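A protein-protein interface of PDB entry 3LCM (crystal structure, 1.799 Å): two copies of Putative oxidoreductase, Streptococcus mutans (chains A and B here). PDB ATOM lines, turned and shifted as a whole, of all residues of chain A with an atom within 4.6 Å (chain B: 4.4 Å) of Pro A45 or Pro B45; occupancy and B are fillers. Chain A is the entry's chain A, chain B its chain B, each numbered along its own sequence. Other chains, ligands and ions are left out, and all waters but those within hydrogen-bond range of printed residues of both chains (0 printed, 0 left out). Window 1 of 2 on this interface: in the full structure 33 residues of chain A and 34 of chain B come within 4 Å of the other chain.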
ATOM      1  N   PHE A  43     -15.230 -32.499   6.519  1.00  0.00           N
ATOM      2  CA  PHE A  43     -14.657 -33.076   5.310  1.00  0.00           C
ATOM      3  C   PHE A  43     -13.411 -32.308   4.867  1.00  0.00           C
ATOM      4  O   PHE A  43     -13.421 -31.081   4.799  1.00  0.00           O
ATOM      5  CB  PHE A  43     -15.698 -33.141   4.179  1.00  0.00           C
ATOM      6  CG  PHE A  43     -15.218 -33.883   2.957  1.00  0.00           C
ATOM      7  CD1 PHE A  43     -15.168 -35.259   2.945  1.00  0.00           C
ATOM      8  CD2 PHE A  43     -14.812 -33.198   1.824  1.00  0.00           C
ATOM      9  CE1 PHE A  43     -14.710 -35.944   1.825  1.00  0.00           C
ATOM     10  CE2 PHE A  43     -14.354 -33.871   0.706  1.00  0.00           C
ATOM     11  CZ  PHE A  43     -14.311 -35.245   0.701  1.00  0.00           C
ATOM     12  N   ASP A  44     -12.336 -33.052   4.600  1.00  0.00           N
ATOM     13  CA  ASP A  44     -11.092 -32.500   4.067  1.00  0.00           C
ATOM     14  C   ASP A  44     -11.129 -32.508   2.535  1.00  0.00           C
ATOM     15  O   ASP A  44     -11.010 -33.568   1.909  1.00  0.00           O
ATOM     16  CB  ASP A  44      -9.893 -33.312   4.577  1.00  0.00           C
ATOM     17  CG  ASP A  44      -8.562 -32.779   4.071  1.00  0.00           C
ATOM     18  OD1 ASP A  44      -8.555 -31.769   3.341  1.00  0.00           O
ATOM     19  OD2 ASP A  44      -7.518 -33.375   4.403  1.00  0.00           O
ATOM     20  N   PRO A  45     -11.287 -31.322   1.925  1.00  0.00           N
ATOM     21  CA  PRO A  45     -11.472 -31.246   0.477  1.00  0.00           C
ATOM     22  C   PRO A  45     -10.167 -31.224  -0.317  1.00  0.00           C
ATOM     23  O   PRO A  45     -10.219 -31.008  -1.523  1.00  0.00           O
ATOM     24  CB  PRO A  45     -12.194 -29.907   0.327  1.00  0.00           C
ATOM     25  CG  PRO A  45     -11.505 -29.061   1.340  1.00  0.00           C
ATOM     26  CD  PRO A  45     -11.461 -29.992   2.547  1.00  0.00           C
ATOM     27  N   VAL A  46      -9.024 -31.442   0.330  1.00  0.00           N
ATOM     28  CA  VAL A  46      -7.740 -31.327  -0.358  1.00  0.00           C
ATOM     29  C   VAL A  46      -7.241 -32.658  -0.924  1.00  0.00           C
ATOM     30  O   VAL A  46      -6.809 -33.541  -0.190  1.00  0.00           O
ATOM     31  CB  VAL A  46      -6.653 -30.659   0.531  1.00  0.00           C
ATOM     32  CG1 VAL A  46      -5.347 -30.521  -0.226  1.00  0.00           C
ATOM     33  CG2 VAL A  46      -7.127 -29.286   1.002  1.00  0.00           C
ATOM     34  N   LEU A  47      -7.311 -32.776  -2.244  1.00  0.00           N
ATOM     35  CA  LEU A  47      -6.797 -33.934  -2.956  1.00  0.00           C
ATOM     36  C   LEU A  47      -5.274 -33.985  -2.861  1.00  0.00           C
ATOM     37  O   LEU A  47      -4.586 -33.003  -3.160  1.00  0.00           O
ATOM     38  CB  LEU A  47      -7.228 -33.873  -4.422  1.00  0.00           C
ATOM     39  CG  LEU A  47      -6.848 -35.020  -5.368  1.00  0.00           C
ATOM     40  CD1 LEU A  47      -7.364 -36.348  -4.837  1.00  0.00           C
ATOM     41  CD2 LEU A  47      -7.389 -34.751  -6.762  1.00  0.00           C
ATOM     42  N   ALA A  90     -15.503 -24.438  -1.892  1.00  0.00           N
ATOM     43  CA  ALA A  90     -14.289 -25.242  -1.968  1.00  0.00           C
ATOM     44  C   ALA A  90     -14.459 -26.620  -1.332  1.00  0.00           C
ATOM     45  O   ALA A  90     -13.936 -27.610  -1.850  1.00  0.00           O
ATOM     46  CB  ALA A  90     -13.109 -24.491  -1.339  1.00  0.00           C
ATOM     47  N   ILE A  91     -15.195 -26.694  -0.222  1.00  0.00           N
ATOM     48  CA  ILE A  91     -15.391 -27.985   0.450  1.00  0.00           C
ATOM     49  C   ILE A  91     -16.145 -28.996  -0.434  1.00  0.00           C
ATOM     50  O   ILE A  91     -15.853 -30.193  -0.394  1.00  0.00           O
ATOM     51  CB  ILE A  91     -16.059 -27.842   1.842  1.00  0.00           C
ATOM     52  CG1 ILE A  91     -15.796 -29.093   2.692  1.00  0.00           C
ATOM     53  CG2 ILE A  91     -17.543 -27.604   1.707  1.00  0.00           C
ATOM     54  CD1 ILE A  91     -16.361 -29.012   4.096  1.00  0.00           C
ATOM     55  N   GLY A  94     -13.916 -30.042  -3.511  1.00  0.00           N
ATOM     56  CA  GLY A  94     -12.991 -31.065  -3.050  1.00  0.00           C
ATOM     57  C   GLY A  94     -13.640 -32.430  -2.842  1.00  0.00           C
ATOM     58  O   GLY A  94     -12.976 -33.460  -2.968  1.00  0.00           O
ATOM     59  N   ARG A  98     -11.878 -35.451  -4.663  1.00  0.00           N
ATOM     60  CA  ARG A  98     -11.382 -36.610  -3.919  1.00  0.00           C
ATOM     61  C   ARG A  98     -12.181 -37.914  -4.093  1.00  0.00           C
ATOM     62  O   ARG A  98     -11.605 -39.002  -4.074  1.00  0.00           O
ATOM     63  CB  ARG A  98     -11.263 -36.266  -2.429  1.00  0.00           C
ATOM     64  CG  ARG A  98     -10.339 -35.098  -2.124  1.00  0.00           C
ATOM     65  CD  ARG A  98      -9.993 -35.075  -0.645  1.00  0.00           C
ATOM     66  NE  ARG A  98      -9.340 -36.316  -0.234  1.00  0.00           N
ATOM     67  CZ  ARG A  98      -9.037 -36.635   1.022  1.00  0.00           C
ATOM     68  NH1 ARG A  98      -9.327 -35.807   2.015  1.00  0.00           N
ATOM     69  NH2 ARG A  98      -8.440 -37.792   1.281  1.00  0.00           N
ATOM     70  N   PHE B  43      -2.539 -24.859   3.453  1.00  0.00           N
ATOM     71  CA  PHE B  43      -3.631 -23.911   3.423  1.00  0.00           C
ATOM     72  C   PHE B  43      -4.957 -24.641   3.632  1.00  0.00           C
ATOM     73  O   PHE B  43      -5.207 -25.701   3.044  1.00  0.00           O
ATOM     74  CB  PHE B  43      -3.637 -23.116   2.110  1.00  0.00           C
ATOM     75  CG  PHE B  43      -4.679 -22.027   2.070  1.00  0.00           C
ATOM     76  CD1 PHE B  43      -4.446 -20.802   2.681  1.00  0.00           C
ATOM     77  CD2 PHE B  43      -5.895 -22.237   1.442  1.00  0.00           C
ATOM     78  CE1 PHE B  43      -5.401 -19.808   2.654  1.00  0.00           C
ATOM     79  CE2 PHE B  43      -6.855 -21.247   1.415  1.00  0.00           C
ATOM     80  CZ  PHE B  43      -6.610 -20.031   2.021  1.00  0.00           C
ATOM     81  N   ASP B  44      -5.781 -24.061   4.498  1.00  0.00           N
ATOM     82  CA  ASP B  44      -7.107 -24.561   4.820  1.00  0.00           C
ATOM     83  C   ASP B  44      -8.126 -23.746   4.035  1.00  0.00           C
ATOM     84  O   ASP B  44      -8.370 -22.577   4.348  1.00  0.00           O
ATOM     85  CB  ASP B  44      -7.349 -24.409   6.318  1.00  0.00           C
ATOM     86  CG  ASP B  44      -8.763 -24.770   6.727  1.00  0.00           C
ATOM     87  OD1 ASP B  44      -9.494 -25.399   5.922  1.00  0.00           O
ATOM     88  OD2 ASP B  44      -9.132 -24.422   7.869  1.00  0.00           O
ATOM     89  N   PRO B  45      -8.726 -24.363   3.010  1.00  0.00           N
ATOM     90  CA  PRO B  45      -9.575 -23.660   2.051  1.00  0.00           C
ATOM     91  C   PRO B  45     -11.051 -23.629   2.442  1.00  0.00           C
ATOM     92  O   PRO B  45     -11.873 -23.133   1.675  1.00  0.00           O
ATOM     93  CB  PRO B  45      -9.390 -24.507   0.794  1.00  0.00           C
ATOM     94  CG  PRO B  45      -9.357 -25.923   1.354  1.00  0.00           C
ATOM     95  CD  PRO B  45      -8.632 -25.804   2.692  1.00  0.00           C
ATOM     96  N   VAL B  46     -11.389 -24.151   3.615  1.00  0.00           N
ATOM     97  CA  VAL B  46     -12.796 -24.247   4.009  1.00  0.00           C
ATOM     98  C   VAL B  46     -13.256 -22.978   4.716  1.00  0.00           C
ATOM     99  O   VAL B  46     -12.833 -22.687   5.839  1.00  0.00           O
ATOM    100  CB  VAL B  46     -13.058 -25.498   4.883  1.00  0.00           C
ATOM    101  CG1 VAL B  46     -14.492 -25.553   5.330  1.00  0.00           C
ATOM    102  CG2 VAL B  46     -12.699 -26.756   4.108  1.00  0.00           C
ATOM    103  N   LEU B  47     -14.112 -22.224   4.031  1.00  0.00           N
ATOM    104  CA  LEU B  47     -14.665 -20.973   4.558  1.00  0.00           C
ATOM    105  C   LEU B  47     -15.674 -21.236   5.668  1.00  0.00           C
ATOM    106  O   LEU B  47     -16.626 -21.983   5.481  1.00  0.00           O
ATOM    107  CB  LEU B  47     -15.321 -20.152   3.437  1.00  0.00           C
ATOM    108  CG  LEU B  47     -15.941 -18.801   3.827  1.00  0.00           C
ATOM    109  CD1 LEU B  47     -14.904 -17.862   4.423  1.00  0.00           C
ATOM    110  CD2 LEU B  47     -16.619 -18.165   2.627  1.00  0.00           C
ATOM    111  N   ALA B  90      -9.646 -27.581  -5.321  1.00  0.00           N
ATOM    112  CA  ALA B  90     -10.383 -27.100  -4.152  1.00  0.00           C
ATOM    113  C   ALA B  90      -9.577 -26.165  -3.238  1.00  0.00           C
ATOM    114  O   ALA B  90     -10.118 -25.200  -2.698  1.00  0.00           O
ATOM    115  CB  ALA B  90     -10.948 -28.294  -3.356  1.00  0.00           C
ATOM    116  N   ILE B  91      -8.287 -26.440  -3.066  1.00  0.00           N
ATOM    117  CA  ILE B  91      -7.464 -25.617  -2.179  1.00  0.00           C
ATOM    118  C   ILE B  91      -7.347 -24.183  -2.705  1.00  0.00           C
ATOM    119  O   ILE B  91      -7.332 -23.228  -1.926  1.00  0.00           O
ATOM    120  CB  ILE B  91      -6.064 -26.249  -1.913  1.00  0.00           C
ATOM    121  CG1 ILE B  91      -5.419 -25.617  -0.673  1.00  0.00           C
ATOM    122  CG2 ILE B  91      -5.177 -26.143  -3.145  1.00  0.00           C
ATOM    123  CD1 ILE B  91      -4.235 -26.399  -0.118  1.00  0.00           C
ATOM    124  N   GLY B  94     -10.727 -22.317  -2.378  1.00  0.00           N
ATOM    125  CA  GLY B  94     -10.926 -21.858  -1.015  1.00  0.00           C
ATOM    126  C   GLY B  94      -9.998 -20.725  -0.657  1.00  0.00           C
ATOM    127  O   GLY B  94     -10.264 -19.962   0.261  1.00  0.00           O
ATOM    128  N   ARG B  98     -11.810 -17.602   0.856  1.00  0.00           N
ATOM    129  CA  ARG B  98     -11.415 -17.123   2.174  1.00  0.00           C
ATOM    130  C   ARG B  98     -10.663 -15.799   2.155  1.00  0.00           C
ATOM    131  O   ARG B  98     -10.747 -15.036   3.110  1.00  0.00           O
ATOM    132  CB  ARG B  98     -10.561 -18.174   2.892  1.00  0.00           C
ATOM    133  CG  ARG B  98     -11.273 -19.478   3.213  1.00  0.00           C
ATOM    134  CD  ARG B  98     -10.486 -20.280   4.252  1.00  0.00           C
ATOM    135  NE  ARG B  98     -10.520 -19.652   5.573  1.00  0.00           N
ATOM    136  CZ  ARG B  98      -9.778 -20.039   6.605  1.00  0.00           C
ATOM    137  NH1 ARG B  98      -8.925 -21.050   6.466  1.00  0.00           N
ATOM    138  NH2 ARG B  98      -9.876 -19.414   7.776  1.00  0.00           N
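N of Val B46 sits at hydrogen-bond distance from OD1 of Asp B44, at 3.2 Å.
Pro B45 touches Pro A45. Pro A45 touches Val B46. Pro A45 touches Ala B90. Ala A90 touches Pro B45 (CB to O, 3.5 Å). Ala A90 touches Ala B90. Ala A90 touches Gly B94. Gly A94 touches Ala B90.
Phe A43 touches none of the printed residues of chain B. Of chain B, only Pro B45, Val B46 and Ala B90 come within 4 Å of Pro A45. Of the printed residues of chain B, Ala A90 touches Pro B45, Ala B90 and Gly B94. Of the printed residues of chain B, Gly A94 touches Ala B90 (3.4 Å). Of the printed residues of chain A, Pro B45 touches Pro A45 (3.8 Å) and Ala A90 (3.5 Å). Of the printed residues of chain A, Val B46 touches Pro A45 (3.8 Å). Printed residues of chain A within 4 Å of Ala B90: Pro A45 (3.4 Å), Ala A90 (3.4 Å) and Gly A94 (3.4 Å). Printed residues of chain A within 4 Å of Gly B94: Ala A90. The nearest printed residue of chain B that does not touch Pro A45 is Ile B91 (5.2 Å).
Hydrophobic or aromatic side chains of chain B within 4 Å of the printed part of chain A: Pro B45, Val B46 and Ala B90. Along chain B the printed residues that touch a printed residue of chain A span positions 45 to 94. Of the 9 printed residues of chain A, 3 touch a printed residue of chain B. Hydrophobic or aromatic side chains of chain A within 4 Å of the printed part of chain B: Pro A45 and Ala A90. Along chain A the printed residues that touch a printed residue of chain B span positions 45 to 94.
Pro B45 touches its own counterpart, Pro A45. Pro A45 touches Ala B90, and with the chains exchanged Ala A90 touches Pro B45. Ala A90 touches its own counterpart, Ala B90. Ala A90 touches Gly B94, and with the chains exchanged Gly A94 touches Ala B90. Positions printed for both chains: 43, 44, 45, 46, 47, 90, 91, 94 and 98. Of the 7 pairs that touch across the chains among the printed residues, 6 have their exchanged pair printed and touching as well.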
